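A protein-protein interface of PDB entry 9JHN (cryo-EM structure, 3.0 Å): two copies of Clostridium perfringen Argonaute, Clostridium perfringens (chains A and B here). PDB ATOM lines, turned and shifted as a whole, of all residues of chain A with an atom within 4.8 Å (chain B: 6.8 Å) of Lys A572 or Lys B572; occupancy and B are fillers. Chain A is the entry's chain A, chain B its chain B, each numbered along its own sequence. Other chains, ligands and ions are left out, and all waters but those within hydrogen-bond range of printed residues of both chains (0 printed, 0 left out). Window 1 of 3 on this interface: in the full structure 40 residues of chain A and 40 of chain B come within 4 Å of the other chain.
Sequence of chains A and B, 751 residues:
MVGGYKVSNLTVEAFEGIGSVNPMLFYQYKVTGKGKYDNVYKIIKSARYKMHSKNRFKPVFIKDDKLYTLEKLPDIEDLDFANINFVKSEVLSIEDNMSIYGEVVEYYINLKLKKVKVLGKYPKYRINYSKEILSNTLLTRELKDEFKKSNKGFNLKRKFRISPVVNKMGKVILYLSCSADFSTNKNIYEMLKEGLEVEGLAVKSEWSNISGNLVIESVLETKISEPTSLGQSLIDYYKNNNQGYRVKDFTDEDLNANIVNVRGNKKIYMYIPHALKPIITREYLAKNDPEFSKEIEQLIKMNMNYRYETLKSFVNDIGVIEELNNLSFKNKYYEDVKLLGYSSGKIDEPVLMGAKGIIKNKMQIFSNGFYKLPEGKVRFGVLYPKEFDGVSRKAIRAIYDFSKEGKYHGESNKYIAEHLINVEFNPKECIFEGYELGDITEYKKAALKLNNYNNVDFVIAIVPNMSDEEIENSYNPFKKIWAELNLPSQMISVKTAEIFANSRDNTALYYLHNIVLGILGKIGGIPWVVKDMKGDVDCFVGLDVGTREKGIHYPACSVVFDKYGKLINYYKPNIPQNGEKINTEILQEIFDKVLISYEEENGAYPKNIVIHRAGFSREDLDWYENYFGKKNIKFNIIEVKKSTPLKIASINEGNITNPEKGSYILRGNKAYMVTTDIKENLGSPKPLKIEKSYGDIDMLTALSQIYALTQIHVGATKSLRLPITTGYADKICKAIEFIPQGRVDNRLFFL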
ATOM      1  N   PRO A 555      17.955  10.335  27.550  1.00  0.00           N
ATOM      2  CA  PRO A 555      19.185  10.783  28.207  1.00  0.00           C
ATOM      3  C   PRO A 555      18.880  11.513  29.503  1.00  0.00           C
ATOM      4  O   PRO A 555      17.791  12.053  29.693  1.00  0.00           O
ATOM      5  CB  PRO A 555      19.817  11.712  27.169  1.00  0.00           C
ATOM      6  CG  PRO A 555      19.276  11.225  25.866  1.00  0.00           C
ATOM      7  CD  PRO A 555      17.879  10.793  26.154  1.00  0.00           C
ATOM      8  N   CYS A 557      18.259  13.906  31.513  1.00  0.00           N
ATOM      9  CA  CYS A 557      17.957  15.326  31.458  1.00  0.00           C
ATOM     10  C   CYS A 557      17.942  15.911  32.857  1.00  0.00           C
ATOM     11  O   CYS A 557      17.162  15.483  33.708  1.00  0.00           O
ATOM     12  CB  CYS A 557      16.611  15.548  30.784  1.00  0.00           C
ATOM     13  SG  CYS A 557      16.580  15.023  29.075  1.00  0.00           S
ATOM     14  N   TYR A 570      19.302  23.811  31.847  1.00  0.00           N
ATOM     15  CA  TYR A 570      19.018  22.396  31.680  1.00  0.00           C
ATOM     16  C   TYR A 570      20.177  21.755  30.941  1.00  0.00           C
ATOM     17  O   TYR A 570      20.765  22.369  30.051  1.00  0.00           O
ATOM     18  CB  TYR A 570      17.697  22.138  30.941  1.00  0.00           C
ATOM     19  CG  TYR A 570      17.598  22.650  29.525  1.00  0.00           C
ATOM     20  CD1 TYR A 570      17.089  23.911  29.264  1.00  0.00           C
ATOM     21  CD2 TYR A 570      17.970  21.856  28.446  1.00  0.00           C
ATOM     22  CE1 TYR A 570      16.979  24.381  27.975  1.00  0.00           C
ATOM     23  CE2 TYR A 570      17.876  22.320  27.158  1.00  0.00           C
ATOM     24  CZ  TYR A 570      17.380  23.584  26.928  1.00  0.00           C
ATOM     25  OH  TYR A 570      17.275  24.053  25.641  1.00  0.00           O
ATOM     26  N   TYR A 571      20.513  20.525  31.305  1.00  0.00           N
ATOM     27  CA  TYR A 571      21.598  19.817  30.645  1.00  0.00           C
ATOM     28  C   TYR A 571      21.090  18.488  30.118  1.00  0.00           C
ATOM     29  O   TYR A 571      20.572  17.672  30.884  1.00  0.00           O
ATOM     30  CB  TYR A 571      22.785  19.597  31.579  1.00  0.00           C
ATOM     31  CG  TYR A 571      23.953  18.979  30.852  1.00  0.00           C
ATOM     32  CD1 TYR A 571      24.709  19.725  29.961  1.00  0.00           C
ATOM     33  CD2 TYR A 571      24.286  17.651  31.036  1.00  0.00           C
ATOM     34  CE1 TYR A 571      25.766  19.167  29.284  1.00  0.00           C
ATOM     35  CE2 TYR A 571      25.344  17.086  30.364  1.00  0.00           C
ATOM     36  CZ  TYR A 571      26.079  17.847  29.491  1.00  0.00           C
ATOM     37  OH  TYR A 571      27.135  17.279  28.823  1.00  0.00           O
ATOM     38  N   LYS A 572      21.249  18.271  28.821  1.00  0.00           N
ATOM     39  CA  LYS A 572      20.912  17.003  28.188  1.00  0.00           C
ATOM     40  C   LYS A 572      22.193  16.397  27.643  1.00  0.00           C
ATOM     41  O   LYS A 572      22.787  16.963  26.709  1.00  0.00           O
ATOM     42  CB  LYS A 572      19.896  17.219  27.067  1.00  0.00           C
ATOM     43  CG  LYS A 572      19.360  15.958  26.392  1.00  0.00           C
ATOM     44  CD  LYS A 572      20.070  15.600  25.090  1.00  0.00           C
ATOM     45  CE  LYS A 572      19.837  16.624  24.012  1.00  0.00           C
ATOM     46  NZ  LYS A 572      20.515  16.254  22.745  1.00  0.00           N
ATOM     47  N   PRO A 573      22.671  15.278  28.184  1.00  0.00           N
ATOM     48  CA  PRO A 573      23.826  14.604  27.585  1.00  0.00           C
ATOM     49  C   PRO A 573      23.480  14.006  26.231  1.00  0.00           C
ATOM     50  O   PRO A 573      22.389  13.477  26.020  1.00  0.00           O
ATOM     51  CB  PRO A 573      24.162  13.515  28.604  1.00  0.00           C
ATOM     52  CG  PRO A 573      23.603  14.009  29.865  1.00  0.00           C
ATOM     53  CD  PRO A 573      22.359  14.736  29.511  1.00  0.00           C
ATOM     54  N   ASN A 574      24.435  14.086  25.307  1.00  0.00           N
ATOM     55  CA  ASN A 574      24.156  13.703  23.929  1.00  0.00           C
ATOM     56  C   ASN A 574      24.100  12.191  23.757  1.00  0.00           C
ATOM     57  O   ASN A 574      23.506  11.697  22.791  1.00  0.00           O
ATOM     58  CB  ASN A 574      25.203  14.307  23.002  1.00  0.00           C
ATOM     59  CG  ASN A 574      25.046  15.797  22.846  1.00  0.00           C
ATOM     60  OD1 ASN A 574      23.940  16.298  22.668  1.00  0.00           O
ATOM     61  ND2 ASN A 574      26.150  16.520  22.927  1.00  0.00           N
ATOM     62  N   ILE A 736      12.107  15.926  23.801  1.00  0.00           N
ATOM     63  CA  ILE A 736      13.538  15.673  23.705  1.00  0.00           C
ATOM     64  C   ILE A 736      14.036  15.837  22.281  1.00  0.00           C
ATOM     65  O   ILE A 736      15.192  16.222  22.078  1.00  0.00           O
ATOM     66  CB  ILE A 736      13.840  14.287  24.307  1.00  0.00           C
ATOM     67  CG1 ILE A 736      15.334  14.037  24.452  1.00  0.00           C
ATOM     68  CG2 ILE A 736      13.167  13.185  23.550  1.00  0.00           C
ATOM     69  CD1 ILE A 736      15.946  14.859  25.497  1.00  0.00           C
ATOM     70  N   ILE A 739      14.481  20.086  21.444  1.00  0.00           N
ATOM     71  CA  ILE A 739      15.403  20.959  22.177  1.00  0.00           C
ATOM     72  C   ILE A 739      16.044  21.937  21.201  1.00  0.00           C
ATOM     73  O   ILE A 739      16.565  21.509  20.156  1.00  0.00           O
ATOM     74  CB  ILE A 739      16.455  20.127  22.906  1.00  0.00           C
ATOM     75  CG1 ILE A 739      15.775  19.257  23.951  1.00  0.00           C
ATOM     76  CG2 ILE A 739      17.483  21.003  23.583  1.00  0.00           C
ATOM     77  CD1 ILE A 739      16.692  18.385  24.699  1.00  0.00           C
ATOM     78  N   PRO B 555      22.972   7.476  18.005  1.00  0.00           N
ATOM     79  CA  PRO B 555      21.850   7.874  17.151  1.00  0.00           C
ATOM     80  C   PRO B 555      22.249   7.871  15.686  1.00  0.00           C
ATOM     81  O   PRO B 555      23.424   7.998  15.343  1.00  0.00           O
ATOM     82  CB  PRO B 555      21.516   9.283  17.647  1.00  0.00           C
ATOM     83  CG  PRO B 555      21.996   9.297  19.059  1.00  0.00           C
ATOM     84  CD  PRO B 555      23.231   8.462  19.066  1.00  0.00           C
ATOM     85  N   ALA B 556      21.253   7.713  14.820  1.00  0.00           N
ATOM     86  CA  ALA B 556      21.494   7.442  13.408  1.00  0.00           C
ATOM     87  C   ALA B 556      22.018   8.689  12.716  1.00  0.00           C
ATOM     88  O   ALA B 556      21.281   9.413  12.046  1.00  0.00           O
ATOM     89  CB  ALA B 556      20.223   6.949  12.734  1.00  0.00           C
ATOM     90  N   CYS B 557      23.314   8.928  12.875  1.00  0.00           N
ATOM     91  CA  CYS B 557      23.950  10.112  12.324  1.00  0.00           C
ATOM     92  C   CYS B 557      24.027  10.009  10.814  1.00  0.00           C
ATOM     93  O   CYS B 557      24.634   9.081  10.278  1.00  0.00           O
ATOM     94  CB  CYS B 557      25.344  10.275  12.910  1.00  0.00           C
ATOM     95  SG  CYS B 557      25.343  10.556  14.676  1.00  0.00           S
ATOM     96  N   SER B 558      23.409  10.959  10.133  1.00  0.00           N
ATOM     97  CA  SER B 558      23.457  11.056   8.685  1.00  0.00           C
ATOM     98  C   SER B 558      24.378  12.199   8.306  1.00  0.00           C
ATOM     99  O   SER B 558      24.533  13.145   9.076  1.00  0.00           O
ATOM    100  CB  SER B 558      22.068  11.291   8.115  1.00  0.00           C
ATOM    101  OG  SER B 558      22.126  11.487   6.724  1.00  0.00           O
ATOM    102  N   TYR B 570      24.658  17.633   8.214  1.00  0.00           N
ATOM    103  CA  TYR B 570      24.602  16.409   8.994  1.00  0.00           C
ATOM    104  C   TYR B 570      23.368  16.450   9.873  1.00  0.00           C
ATOM    105  O   TYR B 570      22.993  17.511  10.372  1.00  0.00           O
ATOM    106  CB  TYR B 570      25.863  16.189   9.845  1.00  0.00           C
ATOM    107  CG  TYR B 570      26.159  17.226  10.902  1.00  0.00           C
ATOM    108  CD1 TYR B 570      26.970  18.313  10.617  1.00  0.00           C
ATOM    109  CD2 TYR B 570      25.668  17.095  12.195  1.00  0.00           C
ATOM    110  CE1 TYR B 570      27.259  19.254  11.578  1.00  0.00           C
ATOM    111  CE2 TYR B 570      25.940  18.033  13.156  1.00  0.00           C
ATOM    112  CZ  TYR B 570      26.737  19.113  12.842  1.00  0.00           C
ATOM    113  OH  TYR B 570      27.022  20.054  13.802  1.00  0.00           O
ATOM    114  N   TYR B 571      22.728  15.305  10.060  1.00  0.00           N
ATOM    115  CA  TYR B 571      21.542  15.237  10.900  1.00  0.00           C
ATOM    116  C   TYR B 571      21.745  14.190  11.979  1.00  0.00           C
ATOM    117  O   TYR B 571      22.010  13.024  11.674  1.00  0.00           O
ATOM    118  CB  TYR B 571      20.287  14.923  10.088  1.00  0.00           C
ATOM    119  CG  TYR B 571      19.046  14.981  10.944  1.00  0.00           C
ATOM    120  CD1 TYR B 571      18.541  16.198  11.378  1.00  0.00           C
ATOM    121  CD2 TYR B 571      18.395  13.828  11.337  1.00  0.00           C
ATOM    122  CE1 TYR B 571      17.421  16.260  12.170  1.00  0.00           C
ATOM    123  CE2 TYR B 571      17.271  13.883  12.127  1.00  0.00           C
ATOM    124  CZ  TYR B 571      16.789  15.098  12.540  1.00  0.00           C
ATOM    125  OH  TYR B 571      15.666  15.148  13.328  1.00  0.00           O
ATOM    126  N   LYS B 572      21.609  14.603  13.230  1.00  0.00           N
ATOM    127  CA  LYS B 572      21.667  13.696  14.368  1.00  0.00           C
ATOM    128  C   LYS B 572      20.309  13.712  15.050  1.00  0.00           C
ATOM    129  O   LYS B 572      19.922  14.753  15.610  1.00  0.00           O
ATOM    130  CB  LYS B 572      22.766  14.127  15.341  1.00  0.00           C
ATOM    131  CG  LYS B 572      23.020  13.199  16.525  1.00  0.00           C
ATOM    132  CD  LYS B 572      22.318  13.622  17.812  1.00  0.00           C
ATOM    133  CE  LYS B 572      22.848  14.924  18.349  1.00  0.00           C
ATOM    134  NZ  LYS B 572      22.172  15.315  19.610  1.00  0.00           N
ATOM    135  N   PRO B 573      19.549  12.621  15.023  1.00  0.00           N
ATOM    136  CA  PRO B 573      18.301  12.573  15.789  1.00  0.00           C
ATOM    137  C   PRO B 573      18.568  12.559  17.286  1.00  0.00           C
ATOM    138  O   PRO B 573      19.510  11.930  17.765  1.00  0.00           O
ATOM    139  CB  PRO B 573      17.658  11.264  15.327  1.00  0.00           C
ATOM    140  CG  PRO B 573      18.250  11.012  14.011  1.00  0.00           C
ATOM    141  CD  PRO B 573      19.649  11.500  14.083  1.00  0.00           C
ATOM    142  N   ASN B 574      17.712  13.258  18.028  1.00  0.00           N
ATOM    143  CA  ASN B 574      17.966  13.457  19.449  1.00  0.00           C
ATOM    144  C   ASN B 574      17.667  12.207  20.263  1.00  0.00           C
ATOM    145  O   ASN B 574      18.178  12.054  21.380  1.00  0.00           O
ATOM    146  CB  ASN B 574      17.147  14.636  19.961  1.00  0.00           C
ATOM    147  CG  ASN B 574      17.665  15.960  19.462  1.00  0.00           C
ATOM    148  OD1 ASN B 574      18.867  16.207  19.467  1.00  0.00           O
ATOM    149  ND2 ASN B 574      16.763  16.815  19.013  1.00  0.00           N
ATOM    150  N   ILE B 575      16.852  11.307  19.732  1.00  0.00           N
ATOM    151  CA  ILE B 575      16.470  10.104  20.474  1.00  0.00           C
ATOM    152  C   ILE B 575      17.354   8.939  20.040  1.00  0.00           C
ATOM    153  O   ILE B 575      17.691   8.834  18.850  1.00  0.00           O
ATOM    154  CB  ILE B 575      14.992   9.785  20.266  1.00  0.00           C
ATOM    155  CG1 ILE B 575      14.613   9.833  18.785  1.00  0.00           C
ATOM    156  CG2 ILE B 575      14.141  10.715  21.056  1.00  0.00           C
ATOM    157  CD1 ILE B 575      13.196   9.409  18.518  1.00  0.00           C
ATOM    158  N   GLU B 589      12.643  11.990   9.440  1.00  0.00           N
ATOM    159  CA  GLU B 589      13.430  13.135   9.902  1.00  0.00           C
ATOM    160  C   GLU B 589      14.690  13.322   9.068  1.00  0.00           C
ATOM    161  O   GLU B 589      14.943  14.415   8.542  1.00  0.00           O
ATOM    162  CB  GLU B 589      13.819  12.946  11.365  1.00  0.00           C
ATOM    163  CG  GLU B 589      12.676  12.892  12.342  1.00  0.00           C
ATOM    164  CD  GLU B 589      13.149  12.605  13.756  1.00  0.00           C
ATOM    165  OE1 GLU B 589      14.364  12.413  13.949  1.00  0.00           O
ATOM    166  OE2 GLU B 589      12.309  12.543  14.674  1.00  0.00           O
ATOM    167  N   ILE B 590      15.456  12.238   8.902  1.00  0.00           N
ATOM    168  CA  ILE B 590      16.737  12.273   8.199  1.00  0.00           C
ATOM    169  C   ILE B 590      16.554  12.700   6.753  1.00  0.00           C
ATOM    170  O   ILE B 590      17.187  13.654   6.298  1.00  0.00           O
ATOM    171  CB  ILE B 590      17.440  10.905   8.298  1.00  0.00           C
ATOM    172  CG1 ILE B 590      18.019  10.689   9.691  1.00  0.00           C
ATOM    173  CG2 ILE B 590      18.515  10.760   7.246  1.00  0.00           C
ATOM    174  CD1 ILE B 590      18.465   9.293   9.928  1.00  0.00           C
ATOM    175  N   LYS B 593      15.309  16.144   6.122  1.00  0.00           N
ATOM    176  CA  LYS B 593      16.421  17.067   6.318  1.00  0.00           C
ATOM    177  C   LYS B 593      17.375  17.055   5.123  1.00  0.00           C
ATOM    178  O   LYS B 593      17.909  18.104   4.746  1.00  0.00           O
ATOM    179  CB  LYS B 593      17.140  16.700   7.612  1.00  0.00           C
ATOM    180  CG  LYS B 593      18.157  17.685   8.084  1.00  0.00           C
ATOM    181  CD  LYS B 593      17.501  18.939   8.597  1.00  0.00           C
ATOM    182  CE  LYS B 593      18.548  19.939   9.041  1.00  0.00           C
ATOM    183  NZ  LYS B 593      19.355  19.412  10.169  1.00  0.00           N
ATOM    184  N   ILE B 732      31.260  11.527  13.403  1.00  0.00           N
ATOM    185  CA  ILE B 732      30.222  12.172  14.201  1.00  0.00           C
ATOM    186  C   ILE B 732      29.771  11.246  15.312  1.00  0.00           C
ATOM    187  O   ILE B 732      29.495  11.689  16.429  1.00  0.00           O
ATOM    188  CB  ILE B 732      29.043  12.613  13.316  1.00  0.00           C
ATOM    189  CG1 ILE B 732      29.489  13.692  12.361  1.00  0.00           C
ATOM    190  CG2 ILE B 732      27.902  13.190  14.130  1.00  0.00           C
ATOM    191  CD1 ILE B 732      28.477  14.043  11.378  1.00  0.00           C
ATOM    192  N   ILE B 736      30.185  12.561  19.277  1.00  0.00           N
ATOM    193  CA  ILE B 736      28.743  12.725  19.393  1.00  0.00           C
ATOM    194  C   ILE B 736      28.378  13.605  20.574  1.00  0.00           C
ATOM    195  O   ILE B 736      27.361  14.304  20.524  1.00  0.00           O
ATOM    196  CB  ILE B 736      28.085  11.332  19.436  1.00  0.00           C
ATOM    197  CG1 ILE B 736      26.568  11.410  19.330  1.00  0.00           C
ATOM    198  CG2 ILE B 736      28.515  10.543  20.635  1.00  0.00           C
ATOM    199  CD1 ILE B 736      26.115  11.816  18.000  1.00  0.00           C
ATOM    200  N   ILE B 739      29.010  17.765  19.456  1.00  0.00           N
ATOM    201  CA  ILE B 739      28.285  18.425  18.366  1.00  0.00           C
ATOM    202  C   ILE B 739      27.952  19.852  18.783  1.00  0.00           C
ATOM    203  O   ILE B 739      27.402  20.058  19.879  1.00  0.00           O
ATOM    204  CB  ILE B 739      27.026  17.636  18.012  1.00  0.00           C
ATOM    205  CG1 ILE B 739      27.419  16.265  17.488  1.00  0.00           C
ATOM    206  CG2 ILE B 739      26.202  18.350  16.965  1.00  0.00           C
ATOM    207  CD1 ILE B 739      26.281  15.402  17.144  1.00  0.00           C
ATOM    208  N   VAL B 744      23.145  23.980  12.171  1.00  0.00           N
ATOM    209  CA  VAL B 744      23.987  22.991  11.511  1.00  0.00           C
ATOM    210  C   VAL B 744      24.391  23.487  10.132  1.00  0.00           C
ATOM    211  O   VAL B 744      23.554  23.940   9.343  1.00  0.00           O
ATOM    212  CB  VAL B 744      23.232  21.655  11.426  1.00  0.00           C
ATOM    213  CG1 VAL B 744      24.058  20.625  10.728  1.00  0.00           C
ATOM    214  CG2 VAL B 744      22.845  21.178  12.806  1.00  0.00           C
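The backbone carbonyl oxygen (O) of Ile A736 lies close to the side-chain amide nitrogen (ND2) of Asn B574. The backbone carbonyl oxygen (O) of Ile B736 sits close to the side-chain amide nitrogen (ND2) of Asn A574 (3.5 Å).
Printed residues of chain B within 4 Å of Lys A572: Lys B572 and Asn B574. Of the printed residues of chain B, Asn A574 touches Lys B572 (3.7 Å) and Ile B736 (3.3 Å). Printed residues of chain B within 4 Å of Ile A736: Asn B574 and Ile B575. Of chain A, only Lys A572 (3.7 Å) and Asn A574 (3.7 Å) come within 4 Å of Lys B572. The nearest printed residue of chain A that does not touch Lys B572 is Pro A573 (6.7 Å).
The side-chain amino group (NZ) of Lys B572 sits at hydrogen-bond distance from the side-chain amide oxygen (OD1) of Asn B574 (3.4 Å). The side-chain amino group of Lys A572 lies within hydrogen-bond range of the side-chain amide oxygen of Asn A574 (3.4 Å).
Lys A572 touches its own counterpart, Lys B572. Lys A572 touches Asn B574, and with the chains exchanged Asn A574 touches Lys B572. Asn A574 touches Ile B736, and with the chains exchanged Ile A736 touches Asn B574. 9 positions are printed for both chains. Of the 6 pairs that touch across the chains among the printed residues, 5 have their exchanged pair printed and touching as well.
Of the 17 printed residues of chain B, 4 touch a printed residue of chain A. Printed residues of chain B that touch a printed residue of chain A: Lys B572, Asn B574, Ile B575 and Ile B736. Hydrophobic or aromatic side chains of chain B that line the printed part of chain A: Ile B575. Along chain B the printed residues that touch a printed residue of chain A span positions 572 to 736. Of the 9 printed residues of chain A, 3 touch a printed residue of chain B. Hydrophobic or aromatic side chains of chain A that line the printed part of chain B: Ile A736. Among the printed residues, no Asp or Glu carboxylate lies within 4 Å of a Lys or Arg side-chain nitrogen of the other chain.
Among the printed residues, merely in contact across the chains: Lys A572 with Lys B572, Lys A572 with Asn B574, Asn A574 with Lys B572 and Ile A736 with Ile B575.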
